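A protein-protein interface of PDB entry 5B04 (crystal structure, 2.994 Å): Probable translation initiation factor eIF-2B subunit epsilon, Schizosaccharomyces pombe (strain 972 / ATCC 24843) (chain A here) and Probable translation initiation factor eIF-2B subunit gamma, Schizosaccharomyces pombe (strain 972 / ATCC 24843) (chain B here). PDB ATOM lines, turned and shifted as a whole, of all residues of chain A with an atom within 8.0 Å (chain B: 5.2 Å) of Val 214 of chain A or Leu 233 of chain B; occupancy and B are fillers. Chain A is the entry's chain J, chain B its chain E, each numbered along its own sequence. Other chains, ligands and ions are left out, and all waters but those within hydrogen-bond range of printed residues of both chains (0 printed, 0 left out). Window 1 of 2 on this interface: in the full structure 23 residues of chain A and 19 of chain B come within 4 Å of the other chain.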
ATOM      1  N   SER A 175      20.526  -0.160   9.163  1.00  0.00           N
ATOM      2  CA  SER A 175      21.374  -0.784   8.158  1.00  0.00           C
ATOM      3  C   SER A 175      21.116  -2.282   8.081  1.00  0.00           C
ATOM      4  O   SER A 175      20.699  -2.901   9.060  1.00  0.00           O
ATOM      5  CB  SER A 175      22.849  -0.522   8.464  1.00  0.00           C
ATOM      6  OG  SER A 175      23.122   0.867   8.525  1.00  0.00           O
ATOM      7  N   VAL A 176      21.367  -2.861   6.911  1.00  0.00           N
ATOM      8  CA  VAL A 176      21.216  -4.297   6.731  1.00  0.00           C
ATOM      9  C   VAL A 176      22.564  -4.996   6.859  1.00  0.00           C
ATOM     10  O   VAL A 176      23.499  -4.707   6.112  1.00  0.00           O
ATOM     11  CB  VAL A 176      20.598  -4.639   5.366  1.00  0.00           C
ATOM     12  CG1 VAL A 176      20.328  -6.133   5.270  1.00  0.00           C
ATOM     13  CG2 VAL A 176      19.316  -3.856   5.161  1.00  0.00           C
ATOM     14  N   PHE A 177      22.656  -5.910   7.818  1.00  0.00           N
ATOM     15  CA  PHE A 177      23.868  -6.691   8.022  1.00  0.00           C
ATOM     16  C   PHE A 177      23.646  -8.138   7.604  1.00  0.00           C
ATOM     17  O   PHE A 177      22.550  -8.675   7.756  1.00  0.00           O
ATOM     18  CB  PHE A 177      24.311  -6.639   9.486  1.00  0.00           C
ATOM     19  CG  PHE A 177      24.828  -5.297   9.926  1.00  0.00           C
ATOM     20  CD1 PHE A 177      23.955  -4.258  10.204  1.00  0.00           C
ATOM     21  CD2 PHE A 177      26.186  -5.082  10.081  1.00  0.00           C
ATOM     22  CE1 PHE A 177      24.427  -3.027  10.615  1.00  0.00           C
ATOM     23  CE2 PHE A 177      26.667  -3.852  10.494  1.00  0.00           C
ATOM     24  CZ  PHE A 177      25.786  -2.823  10.761  1.00  0.00           C
ATOM     25  N   VAL A 178      24.689  -8.763   7.068  1.00  0.00           N
ATOM     26  CA  VAL A 178      24.668 -10.197   6.818  1.00  0.00           C
ATOM     27  C   VAL A 178      25.868 -10.827   7.508  1.00  0.00           C
ATOM     28  O   VAL A 178      27.013 -10.588   7.127  1.00  0.00           O
ATOM     29  CB  VAL A 178      24.693 -10.530   5.317  1.00  0.00           C
ATOM     30  CG1 VAL A 178      24.709 -12.037   5.111  1.00  0.00           C
ATOM     31  CG2 VAL A 178      23.496  -9.908   4.615  1.00  0.00           C
ATOM     32  N   ILE A 179      25.599 -11.623   8.537  1.00  0.00           N
ATOM     33  CA  ILE A 179      26.657 -12.152   9.385  1.00  0.00           C
ATOM     34  C   ILE A 179      26.704 -13.676   9.365  1.00  0.00           C
ATOM     35  O   ILE A 179      25.670 -14.338   9.455  1.00  0.00           O
ATOM     36  CB  ILE A 179      26.486 -11.679  10.843  1.00  0.00           C
ATOM     37  CG1 ILE A 179      25.922 -10.256  10.884  1.00  0.00           C
ATOM     38  CG2 ILE A 179      27.802 -11.761  11.591  1.00  0.00           C
ATOM     39  CD1 ILE A 179      25.658  -9.746  12.282  1.00  0.00           C
ATOM     40  N   ASP A 180      27.910 -14.224   9.240  1.00  0.00           N
ATOM     41  CA  ASP A 180      28.119 -15.662   9.358  1.00  0.00           C
ATOM     42  C   ASP A 180      27.725 -16.090  10.766  1.00  0.00           C
ATOM     43  O   ASP A 180      28.331 -15.659  11.744  1.00  0.00           O
ATOM     44  CB  ASP A 180      29.577 -16.022   9.053  1.00  0.00           C
ATOM     45  CG  ASP A 180      29.820 -17.524   8.998  1.00  0.00           C
ATOM     46  OD1 ASP A 180      29.481 -18.234   9.968  1.00  0.00           O
ATOM     47  OD2 ASP A 180      30.361 -17.995   7.975  1.00  0.00           O
ATOM     48  N   LYS A 181      26.710 -16.942  10.861  1.00  0.00           N
ATOM     49  CA  LYS A 181      26.103 -17.276  12.146  1.00  0.00           C
ATOM     50  C   LYS A 181      27.059 -17.955  13.126  1.00  0.00           C
ATOM     51  O   LYS A 181      26.824 -17.935  14.333  1.00  0.00           O
ATOM     52  CB  LYS A 181      24.874 -18.163  11.930  1.00  0.00           C
ATOM     53  CG  LYS A 181      23.776 -17.501  11.114  1.00  0.00           C
ATOM     54  CD  LYS A 181      22.494 -18.313  11.142  1.00  0.00           C
ATOM     55  CE  LYS A 181      21.903 -18.352  12.541  1.00  0.00           C
ATOM     56  NZ  LYS A 181      20.568 -19.010  12.563  1.00  0.00           N
ATOM     57  N   VAL A 187      29.766 -10.188   6.312  1.00  0.00           N
ATOM     58  CA  VAL A 187      30.074 -10.415   4.905  1.00  0.00           C
ATOM     59  C   VAL A 187      29.268  -9.486   4.001  1.00  0.00           C
ATOM     60  O   VAL A 187      29.416  -9.517   2.779  1.00  0.00           O
ATOM     61  CB  VAL A 187      29.806 -11.876   4.493  1.00  0.00           C
ATOM     62  CG1 VAL A 187      30.639 -12.826   5.342  1.00  0.00           C
ATOM     63  CG2 VAL A 187      28.327 -12.202   4.612  1.00  0.00           C
ATOM     64  N   HIS A 188      28.418  -8.662   4.606  1.00  0.00           N
ATOM     65  CA  HIS A 188      27.642  -7.682   3.854  1.00  0.00           C
ATOM     66  C   HIS A 188      27.103  -6.573   4.751  1.00  0.00           C
ATOM     67  O   HIS A 188      26.569  -6.830   5.831  1.00  0.00           O
ATOM     68  CB  HIS A 188      26.483  -8.358   3.116  1.00  0.00           C
ATOM     69  CG  HIS A 188      25.745  -7.448   2.182  1.00  0.00           C
ATOM     70  ND1 HIS A 188      25.772  -7.608   0.814  1.00  0.00           N
ATOM     71  CD2 HIS A 188      24.960  -6.370   2.419  1.00  0.00           C
ATOM     72  CE1 HIS A 188      25.036  -6.668   0.248  1.00  0.00           C
ATOM     73  NE2 HIS A 188      24.533  -5.903   1.200  1.00  0.00           N
ATOM     74  N   GLN A 190      24.943  -2.666   4.207  1.00  0.00           N
ATOM     75  CA  GLN A 190      24.375  -1.617   3.374  1.00  0.00           C
ATOM     76  C   GLN A 190      23.447  -0.732   4.197  1.00  0.00           C
ATOM     77  O   GLN A 190      22.521  -1.216   4.850  1.00  0.00           O
ATOM     78  CB  GLN A 190      23.638  -2.207   2.167  1.00  0.00           C
ATOM     79  CG  GLN A 190      22.546  -3.211   2.499  1.00  0.00           C
ATOM     80  CD  GLN A 190      21.685  -3.543   1.297  1.00  0.00           C
ATOM     81  OE1 GLN A 190      21.974  -4.479   0.552  1.00  0.00           O
ATOM     82  NE2 GLN A 190      20.624  -2.771   1.098  1.00  0.00           N
ATOM     83  N   VAL A 199      18.561  -5.943  -1.631  1.00  0.00           N
ATOM     84  CA  VAL A 199      19.810  -6.360  -1.011  1.00  0.00           C
ATOM     85  C   VAL A 199      20.582  -7.221  -2.003  1.00  0.00           C
ATOM     86  O   VAL A 199      20.230  -8.377  -2.238  1.00  0.00           O
ATOM     87  CB  VAL A 199      19.575  -7.153   0.288  1.00  0.00           C
ATOM     88  CG1 VAL A 199      20.899  -7.624   0.871  1.00  0.00           C
ATOM     89  CG2 VAL A 199      18.812  -6.309   1.296  1.00  0.00           C
ATOM     90  N   MET A 201      23.695  -9.270  -2.950  1.00  0.00           N
ATOM     91  CA  MET A 201      24.886  -9.981  -2.503  1.00  0.00           C
ATOM     92  C   MET A 201      25.582 -10.672  -3.670  1.00  0.00           C
ATOM     93  O   MET A 201      24.930 -11.170  -4.587  1.00  0.00           O
ATOM     94  CB  MET A 201      24.534 -11.009  -1.428  1.00  0.00           C
ATOM     95  CG  MET A 201      24.056 -10.413  -0.115  1.00  0.00           C
ATOM     96  SD  MET A 201      23.675 -11.682   1.108  1.00  0.00           S
ATOM     97  CE  MET A 201      25.267 -12.486   1.267  1.00  0.00           C
ATOM     98  N   PHE A 206      28.486 -17.335  -0.778  1.00  0.00           N
ATOM     99  CA  PHE A 206      27.701 -18.501  -0.371  1.00  0.00           C
ATOM    100  C   PHE A 206      28.422 -19.844  -0.432  1.00  0.00           C
ATOM    101  O   PHE A 206      27.949 -20.821   0.154  1.00  0.00           O
ATOM    102  CB  PHE A 206      26.430 -18.585  -1.218  1.00  0.00           C
ATOM    103  CG  PHE A 206      25.420 -17.529  -0.889  1.00  0.00           C
ATOM    104  CD1 PHE A 206      25.128 -17.232   0.432  1.00  0.00           C
ATOM    105  CD2 PHE A 206      24.761 -16.834  -1.889  1.00  0.00           C
ATOM    106  CE1 PHE A 206      24.203 -16.266   0.750  1.00  0.00           C
ATOM    107  CE2 PHE A 206      23.835 -15.861  -1.574  1.00  0.00           C
ATOM    108  CZ  PHE A 206      23.555 -15.578  -0.251  1.00  0.00           C
ATOM    109  N   HIS A 209      30.727 -19.245   3.058  1.00  0.00           N
ATOM    110  CA  HIS A 209      29.898 -18.958   4.227  1.00  0.00           C
ATOM    111  C   HIS A 209      28.519 -19.497   3.944  1.00  0.00           C
ATOM    112  O   HIS A 209      27.923 -19.163   2.920  1.00  0.00           O
ATOM    113  CB  HIS A 209      29.813 -17.466   4.520  1.00  0.00           C
ATOM    114  CG  HIS A 209      31.138 -16.805   4.696  1.00  0.00           C
ATOM    115  ND1 HIS A 209      31.908 -16.975   5.825  1.00  0.00           N
ATOM    116  CD2 HIS A 209      31.821 -15.957   3.894  1.00  0.00           C
ATOM    117  CE1 HIS A 209      33.017 -16.269   5.706  1.00  0.00           C
ATOM    118  NE2 HIS A 209      32.988 -15.640   4.543  1.00  0.00           N
ATOM    119  N   GLU A 210      27.986 -20.321   4.833  1.00  0.00           N
ATOM    120  CA  GLU A 210      26.836 -21.078   4.399  1.00  0.00           C
ATOM    121  C   GLU A 210      25.615 -21.112   5.303  1.00  0.00           C
ATOM    122  O   GLU A 210      24.531 -21.523   4.877  1.00  0.00           O
ATOM    123  CB  GLU A 210      27.280 -22.490   4.080  1.00  0.00           C
ATOM    124  CG  GLU A 210      27.066 -22.720   2.629  1.00  0.00           C
ATOM    125  CD  GLU A 210      25.602 -22.600   2.336  1.00  0.00           C
ATOM    126  OE1 GLU A 210      24.919 -23.614   2.536  1.00  0.00           O
ATOM    127  OE2 GLU A 210      25.125 -21.499   1.969  1.00  0.00           O
ATOM    128  N   GLU A 211      25.777 -20.680   6.543  1.00  0.00           N
ATOM    129  CA  GLU A 211      24.620 -20.272   7.315  1.00  0.00           C
ATOM    130  C   GLU A 211      24.807 -18.809   7.668  1.00  0.00           C
ATOM    131  O   GLU A 211      25.427 -18.461   8.672  1.00  0.00           O
ATOM    132  CB  GLU A 211      24.417 -21.152   8.547  1.00  0.00           C
ATOM    133  CG  GLU A 211      23.978 -22.559   8.168  1.00  0.00           C
ATOM    134  CD  GLU A 211      23.620 -23.426   9.357  1.00  0.00           C
ATOM    135  OE1 GLU A 211      22.697 -23.052  10.109  1.00  0.00           O
ATOM    136  OE2 GLU A 211      24.251 -24.488   9.527  1.00  0.00           O
ATOM    137  N   LEU A 212      24.297 -17.961   6.780  1.00  0.00           N
ATOM    138  CA  LEU A 212      24.348 -16.519   6.946  1.00  0.00           C
ATOM    139  C   LEU A 212      23.042 -16.024   7.535  1.00  0.00           C
ATOM    140  O   LEU A 212      22.006 -16.677   7.405  1.00  0.00           O
ATOM    141  CB  LEU A 212      24.616 -15.828   5.607  1.00  0.00           C
ATOM    142  CG  LEU A 212      25.969 -16.106   4.955  1.00  0.00           C
ATOM    143  CD1 LEU A 212      26.082 -15.385   3.623  1.00  0.00           C
ATOM    144  CD2 LEU A 212      27.079 -15.679   5.891  1.00  0.00           C
ATOM    145  N   GLU A 213      23.091 -14.869   8.185  1.00  0.00           N
ATOM    146  CA  GLU A 213      21.889 -14.278   8.745  1.00  0.00           C
ATOM    147  C   GLU A 213      21.734 -12.831   8.301  1.00  0.00           C
ATOM    148  O   GLU A 213      22.523 -11.965   8.680  1.00  0.00           O
ATOM    149  CB  GLU A 213      21.905 -14.362  10.271  1.00  0.00           C
ATOM    150  CG  GLU A 213      20.601 -13.928  10.911  1.00  0.00           C
ATOM    151  CD  GLU A 213      20.569 -14.173  12.404  1.00  0.00           C
ATOM    152  OE1 GLU A 213      21.652 -14.310  13.012  1.00  0.00           O
ATOM    153  OE2 GLU A 213      19.458 -14.234  12.968  1.00  0.00           O
ATOM    154  N   VAL A 214      20.718 -12.582   7.484  1.00  0.00           N
ATOM    155  CA  VAL A 214      20.396 -11.228   7.060  1.00  0.00           C
ATOM    156  C   VAL A 214      19.633 -10.530   8.178  1.00  0.00           C
ATOM    157  O   VAL A 214      18.591 -11.014   8.619  1.00  0.00           O
ATOM    158  CB  VAL A 214      19.557 -11.220   5.773  1.00  0.00           C
ATOM    159  CG1 VAL A 214      19.801  -9.938   4.998  1.00  0.00           C
ATOM    160  CG2 VAL A 214      19.892 -12.430   4.916  1.00  0.00           C
ATOM    161  N   ARG A 215      20.155  -9.400   8.642  1.00  0.00           N
ATOM    162  CA  ARG A 215      19.576  -8.736   9.804  1.00  0.00           C
ATOM    163  C   ARG A 215      19.215  -7.278   9.536  1.00  0.00           C
ATOM    164  O   ARG A 215      20.073  -6.456   9.213  1.00  0.00           O
ATOM    165  CB  ARG A 215      20.537  -8.826  10.991  1.00  0.00           C
ATOM    166  CG  ARG A 215      21.000 -10.244  11.291  1.00  0.00           C
ATOM    167  CD  ARG A 215      21.535 -10.379  12.703  1.00  0.00           C
ATOM    168  NE  ARG A 215      20.495 -10.147  13.701  1.00  0.00           N
ATOM    169  CZ  ARG A 215      20.564 -10.561  14.961  1.00  0.00           C
ATOM    170  NH1 ARG A 215      21.624 -11.239  15.381  1.00  0.00           N
ATOM    171  NH2 ARG A 215      19.570 -10.306  15.800  1.00  0.00           N
ATOM    172  N   ASN A 216      17.928  -6.975   9.677  1.00  0.00           N
ATOM    173  CA  ASN A 216      17.418  -5.617   9.540  1.00  0.00           C
ATOM    174  C   ASN A 216      16.919  -5.122  10.897  1.00  0.00           C
ATOM    175  O   ASN A 216      16.194  -4.132  10.994  1.00  0.00           O
ATOM    176  CB  ASN A 216      16.301  -5.575   8.492  1.00  0.00           C
ATOM    177  CG  ASN A 216      15.855  -4.163   8.161  1.00  0.00           C
ATOM    178  OD1 ASN A 216      16.622  -3.209   8.289  1.00  0.00           O
ATOM    179  ND2 ASN A 216      14.604  -4.024   7.738  1.00  0.00           N
ATOM    180  N   ASP A 217      17.325  -5.823  11.950  1.00  0.00           N
ATOM    181  CA  ASP A 217      16.847  -5.535  13.297  1.00  0.00           C
ATOM    182  C   ASP A 217      17.915  -4.888  14.172  1.00  0.00           C
ATOM    183  O   ASP A 217      17.685  -4.627  15.350  1.00  0.00           O
ATOM    184  CB  ASP A 217      16.354  -6.821  13.965  1.00  0.00           C
ATOM    185  CG  ASP A 217      17.477  -7.809  14.222  1.00  0.00           C
ATOM    186  OD1 ASP A 217      18.285  -8.049  13.300  1.00  0.00           O
ATOM    187  OD2 ASP A 217      17.556  -8.342  15.349  1.00  0.00           O
ATOM    188  N   LEU A 218      19.082  -4.625  13.597  1.00  0.00           N
ATOM    189  CA  LEU A 218      20.216  -4.151  14.383  1.00  0.00           C
ATOM    190  C   LEU A 218      20.253  -2.634  14.536  1.00  0.00           C
ATOM    191  O   LEU A 218      19.742  -1.896  13.694  1.00  0.00           O
ATOM    192  CB  LEU A 218      21.523  -4.635  13.755  1.00  0.00           C
ATOM    193  CG  LEU A 218      21.701  -6.152  13.680  1.00  0.00           C
ATOM    194  CD1 LEU A 218      23.011  -6.504  12.995  1.00  0.00           C
ATOM    195  CD2 LEU A 218      21.631  -6.767  15.069  1.00  0.00           C
ATOM    196  N   LEU B 195      19.572 -22.410  -2.603  1.00  0.00           N
ATOM    197  CA  LEU B 195      19.646 -21.581  -1.406  1.00  0.00           C
ATOM    198  C   LEU B 195      18.273 -21.392  -0.769  1.00  0.00           C
ATOM    199  O   LEU B 195      17.321 -20.977  -1.428  1.00  0.00           O
ATOM    200  CB  LEU B 195      20.270 -20.227  -1.742  1.00  0.00           C
ATOM    201  CG  LEU B 195      20.302 -19.155  -0.653  1.00  0.00           C
ATOM    202  CD1 LEU B 195      20.819 -19.694   0.660  1.00  0.00           C
ATOM    203  CD2 LEU B 195      21.184 -18.029  -1.114  1.00  0.00           C
ATOM    204  N   ILE B 196      18.188 -21.695   0.524  1.00  0.00           N
ATOM    205  CA  ILE B 196      16.928 -21.623   1.252  1.00  0.00           C
ATOM    206  C   ILE B 196      17.000 -20.653   2.428  1.00  0.00           C
ATOM    207  O   ILE B 196      17.788 -20.841   3.356  1.00  0.00           O
ATOM    208  CB  ILE B 196      16.512 -23.011   1.775  1.00  0.00           C
ATOM    209  CG1 ILE B 196      16.337 -23.987   0.610  1.00  0.00           C
ATOM    210  CG2 ILE B 196      15.234 -22.914   2.588  1.00  0.00           C
ATOM    211  CD1 ILE B 196      15.365 -23.507  -0.444  1.00  0.00           C
ATOM    212  N   GLY B 197      16.171 -19.615   2.381  1.00  0.00           N
ATOM    213  CA  GLY B 197      16.095 -18.647   3.459  1.00  0.00           C
ATOM    214  C   GLY B 197      14.851 -18.840   4.305  1.00  0.00           C
ATOM    215  O   GLY B 197      13.740 -18.568   3.854  1.00  0.00           O
ATOM    216  N   TYR B 207      12.930 -17.336   1.317  1.00  0.00           N
ATOM    217  CA  TYR B 207      13.556 -17.418   0.001  1.00  0.00           C
ATOM    218  C   TYR B 207      13.833 -18.874  -0.346  1.00  0.00           C
ATOM    219  O   TYR B 207      14.251 -19.652   0.511  1.00  0.00           O
ATOM    220  CB  TYR B 207      14.847 -16.603  -0.051  1.00  0.00           C
ATOM    221  CG  TYR B 207      15.265 -16.245  -1.459  1.00  0.00           C
ATOM    222  CD1 TYR B 207      15.919 -17.167  -2.266  1.00  0.00           C
ATOM    223  CD2 TYR B 207      14.995 -14.990  -1.986  1.00  0.00           C
ATOM    224  CE1 TYR B 207      16.294 -16.848  -3.555  1.00  0.00           C
ATOM    225  CE2 TYR B 207      15.369 -14.660  -3.275  1.00  0.00           C
ATOM    226  CZ  TYR B 207      16.018 -15.593  -4.055  1.00  0.00           C
ATOM    227  OH  TYR B 207      16.392 -15.270  -5.338  1.00  0.00           O
ATOM    228  N   PHE B 220      17.290  -9.768  -2.361  1.00  0.00           N
ATOM    229  CA  PHE B 220      16.167  -9.863  -1.458  1.00  0.00           C
ATOM    230  C   PHE B 220      15.519  -8.506  -1.488  1.00  0.00           C
ATOM    231  O   PHE B 220      16.202  -7.510  -1.386  1.00  0.00           O
ATOM    232  CB  PHE B 220      16.630 -10.129  -0.040  1.00  0.00           C
ATOM    233  CG  PHE B 220      17.490 -11.336   0.103  1.00  0.00           C
ATOM    234  CD1 PHE B 220      18.787 -11.330  -0.344  1.00  0.00           C
ATOM    235  CD2 PHE B 220      17.005 -12.473   0.696  1.00  0.00           C
ATOM    236  CE1 PHE B 220      19.588 -12.446  -0.211  1.00  0.00           C
ATOM    237  CE2 PHE B 220      17.797 -13.592   0.831  1.00  0.00           C
ATOM    238  CZ  PHE B 220      19.093 -13.580   0.379  1.00  0.00           C
ATOM    239  N   LEU B 225      12.055  -7.482   4.132  1.00  0.00           N
ATOM    240  CA  LEU B 225      12.913  -7.502   5.320  1.00  0.00           C
ATOM    241  C   LEU B 225      12.537  -6.470   6.386  1.00  0.00           C
ATOM    242  O   LEU B 225      13.159  -6.422   7.448  1.00  0.00           O
ATOM    243  CB  LEU B 225      14.378  -7.305   4.932  1.00  0.00           C
ATOM    244  CG  LEU B 225      15.284  -8.531   5.091  1.00  0.00           C
ATOM    245  CD1 LEU B 225      15.006  -9.584   4.030  1.00  0.00           C
ATOM    246  CD2 LEU B 225      16.747  -8.119   5.084  1.00  0.00           C
ATOM    247  N   PRO B 229      12.537  -9.321  10.082  1.00  0.00           N
ATOM    248  CA  PRO B 229      13.842  -8.645  10.058  1.00  0.00           C
ATOM    249  C   PRO B 229      15.033  -9.598  10.052  1.00  0.00           C
ATOM    250  O   PRO B 229      16.146  -9.184   9.726  1.00  0.00           O
ATOM    251  CB  PRO B 229      13.833  -7.818  11.346  1.00  0.00           C
ATOM    252  CG  PRO B 229      12.864  -8.510  12.236  1.00  0.00           C
ATOM    253  CD  PRO B 229      11.804  -9.060  11.332  1.00  0.00           C
ATOM    254  N   ARG B 230      14.800 -10.857  10.410  1.00  0.00           N
ATOM    255  CA  ARG B 230      15.873 -11.839  10.491  1.00  0.00           C
ATOM    256  C   ARG B 230      15.610 -13.040   9.591  1.00  0.00           C
ATOM    257  O   ARG B 230      14.595 -13.722   9.732  1.00  0.00           O
ATOM    258  CB  ARG B 230      16.057 -12.298  11.936  1.00  0.00           C
ATOM    259  CG  ARG B 230      16.241 -11.160  12.925  1.00  0.00           C
ATOM    260  CD  ARG B 230      16.495 -11.690  14.322  1.00  0.00           C
ATOM    261  NE  ARG B 230      17.584 -12.660  14.334  1.00  0.00           N
ATOM    262  CZ  ARG B 230      18.032 -13.267  15.427  1.00  0.00           C
ATOM    263  NH1 ARG B 230      17.485 -13.006  16.606  1.00  0.00           N
ATOM    264  NH2 ARG B 230      19.029 -14.136  15.339  1.00  0.00           N
ATOM    265  N   VAL B 231      16.530 -13.290   8.662  1.00  0.00           N
ATOM    266  CA  VAL B 231      16.416 -14.422   7.748  1.00  0.00           C
ATOM    267  C   VAL B 231      17.697 -15.254   7.748  1.00  0.00           C
ATOM    268  O   VAL B 231      18.794 -14.715   7.611  1.00  0.00           O
ATOM    269  CB  VAL B 231      16.120 -13.965   6.303  1.00  0.00           C
ATOM    270  CG1 VAL B 231      15.786 -15.163   5.426  1.00  0.00           C
ATOM    271  CG2 VAL B 231      14.988 -12.949   6.278  1.00  0.00           C
ATOM    272  N   THR B 232      17.551 -16.566   7.901  1.00  0.00           N
ATOM    273  CA  THR B 232      18.692 -17.475   7.891  1.00  0.00           C
ATOM    274  C   THR B 232      18.883 -18.106   6.513  1.00  0.00           C
ATOM    275  O   THR B 232      17.969 -18.731   5.981  1.00  0.00           O
ATOM    276  CB  THR B 232      18.530 -18.593   8.942  1.00  0.00           C
ATOM    277  OG1 THR B 232      18.687 -18.044  10.257  1.00  0.00           O
ATOM    278  CG2 THR B 232      19.570 -19.682   8.732  1.00  0.00           C
ATOM    279  N   LEU B 233      20.075 -17.942   5.944  1.00  0.00           N
ATOM    280  CA  LEU B 233      20.372 -18.470   4.614  1.00  0.00           C
ATOM    281  C   LEU B 233      21.109 -19.812   4.665  1.00  0.00           C
ATOM    282  O   LEU B 233      21.934 -20.048   5.546  1.00  0.00           O
ATOM    283  CB  LEU B 233      21.184 -17.451   3.814  1.00  0.00           C
ATOM    284  CG  LEU B 233      20.407 -16.204   3.389  1.00  0.00           C
ATOM    285  CD1 LEU B 233      21.308 -15.219   2.660  1.00  0.00           C
ATOM    286  CD2 LEU B 233      19.221 -16.598   2.523  1.00  0.00           C
ATOM    287  N   ASN B 234      20.802 -20.677   3.699  1.00  0.00           N
ATOM    288  CA  ASN B 234      21.308 -22.049   3.657  1.00  0.00           C
ATOM    289  C   ASN B 234      21.371 -22.631   2.237  1.00  0.00           C
ATOM    290  O   ASN B 234      20.333 -22.967   1.672  1.00  0.00           O
ATOM    291  CB  ASN B 234      20.419 -22.960   4.516  1.00  0.00           C
ATOM    292  CG  ASN B 234      20.921 -23.117   5.939  1.00  0.00           C
ATOM    293  OD1 ASN B 234      21.879 -23.845   6.193  1.00  0.00           O
ATOM    294  ND2 ASN B 234      20.252 -22.458   6.879  1.00  0.00           N
ATOM    295  N   THR B 235      22.565 -22.752   1.653  1.00  0.00           N
ATOM    296  CA  THR B 235      22.705 -23.570   0.442  1.00  0.00           C
ATOM    297  C   THR B 235      23.201 -24.954   0.851  1.00  0.00           C
ATOM    298  O   THR B 235      23.634 -25.751   0.021  1.00  0.00           O
ATOM    299  CB  THR B 235      23.670 -22.963  -0.626  1.00  0.00           C
ATOM    300  OG1 THR B 235      25.017 -23.387  -0.379  1.00  0.00           O
ATOM    301  CG2 THR B 235      23.590 -21.443  -0.669  1.00  0.00           C
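Val 214 of chain A touches five residues of chain B.
Of the printed residues of chain A, Val 231 of chain B touches Leu 212 (3.8 Å), Glu 213 (3.3 Å) and Val 214 (2.9 Å).
Printed residues of chain A within 4 Å of Thr 232 of chain B: Lys 181 and Leu 212.
His 188 of chain A touches none of the printed residues of chain B.
The nearest residue of chain A that does not touch Leu 233 of chain B is Met 201 of chain A (4.5 Å).
Among the printed residues, merely in contact across the chains: Glu 211 of chain A with Asn 234 of chain B (3.2 Å), Glu 211 of chain A with Leu 233 of chain B (3.2 Å), Glu 213 of chain A with Val 231 of chain B (3.3 Å), Val 214 of chain A with Arg 230 of chain B (3.4 Å), Leu 212 of chain A with Thr 232 of chain B (3.4 Å), Phe 206 of chain A with Leu 195 of chain B (3.5 Å), Arg 215 of chain A with Pro 229 of chain B (3.5 Å), Glu 210 of chain A with Asn 234 of chain B (3.5 Å), Val 214 of chain A with Leu 225 of chain B (3.6 Å), Phe 206 of chain A with Leu 233 of chain B (3.6 Å), Asp 217 of chain A with Arg 230 of chain B (3.7 Å), Asp 217 of chain A with Pro 229 of chain B (3.8 Å), Leu 212 of chain A with Val 231 of chain B (3.8 Å), Val 214 of chain A with Leu 233 of chain B (3.9 Å) and Phe 206 of chain A with Thr 235 of chain B (3.9 Å).
Of the 23 printed residues of chain A, 11 touch a printed residue of chain B.
Among the printed residues, Asp or Glu carboxylates within 4 Å of a Lys or Arg side-chain nitrogen of the other chain: Glu 213 of chain A with Arg 230 of chain B (2.4 Å).
The backbone carbonyl oxygen (O) of Ile 179 of chain A sits at hydrogen-bond distance from the backbone NH (N) of Glu 213 of chain A (2.9 Å).
N of Arg 215 of chain A sits at hydrogen-bond distance from O of Phe 177 of chain A, at 2.7 Å.
NH1 of Arg 215 of chain A lies within salt-bridge range of OE1 of Glu 213 of chain A (3.9 Å).
The backbone carbonyl oxygen (O) of Asn 234 of chain B sits at hydrogen-bond distance from the backbone NH (N) of Ile 196 of chain B (2.7 Å).
OD2 of Asp 217 of chain A lies within salt-bridge range of NH2 of Arg 215 of chain A (2.8 Å).
O of Glu 210 of chain A lies close to O of Leu 233 of chain B (3.1 Å).
O of Pro 229 of chain B is in hydrogen-bond range of N of Asn 216 of chain A, at 2.8 Å.
The backbone carbonyl oxygen (O) of Leu 225 of chain B sits at hydrogen-bond distance from the side-chain amide nitrogen (ND2) of Asn 216 of chain A (2.8 Å).
O of Leu 212 of chain A is in hydrogen-bond range of N of Leu 233 of chain B (2.7 Å).
The backbone NH (N) of Val 214 of chain A is in hydrogen-bond range of the backbone carbonyl oxygen (O) of Val 231 of chain B (2.9 Å).
The guanidinium group (NH2) of Arg 215 of chain A sits close to the guanidinium group (NE) of Arg 230 of chain B (3.4 Å).
The backbone carbonyl oxygen (O) of Val 214 of chain A sits close to the backbone carbonyl oxygen (O) of Pro 229 of chain B (3.2 Å).
The backbone NH of Thr 235 of chain B is in hydrogen-bond range of the side-chain carboxylate of Glu 210 of chain A (2.7 Å).
The backbone carbonyl oxygen (O) of Phe 220 of chain B lies within hydrogen-bond range of the backbone NH (N) of Val 199 of chain A (2.8 Å).
The guanidinium group (NH2) of Arg 230 of chain B lies within salt-bridge range of the side-chain carboxylate (OE2) of Glu 213 of chain A (2.4 Å).
OG1 of Thr 232 of chain B is in hydrogen-bond range of NZ of Lys 181 of chain A.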
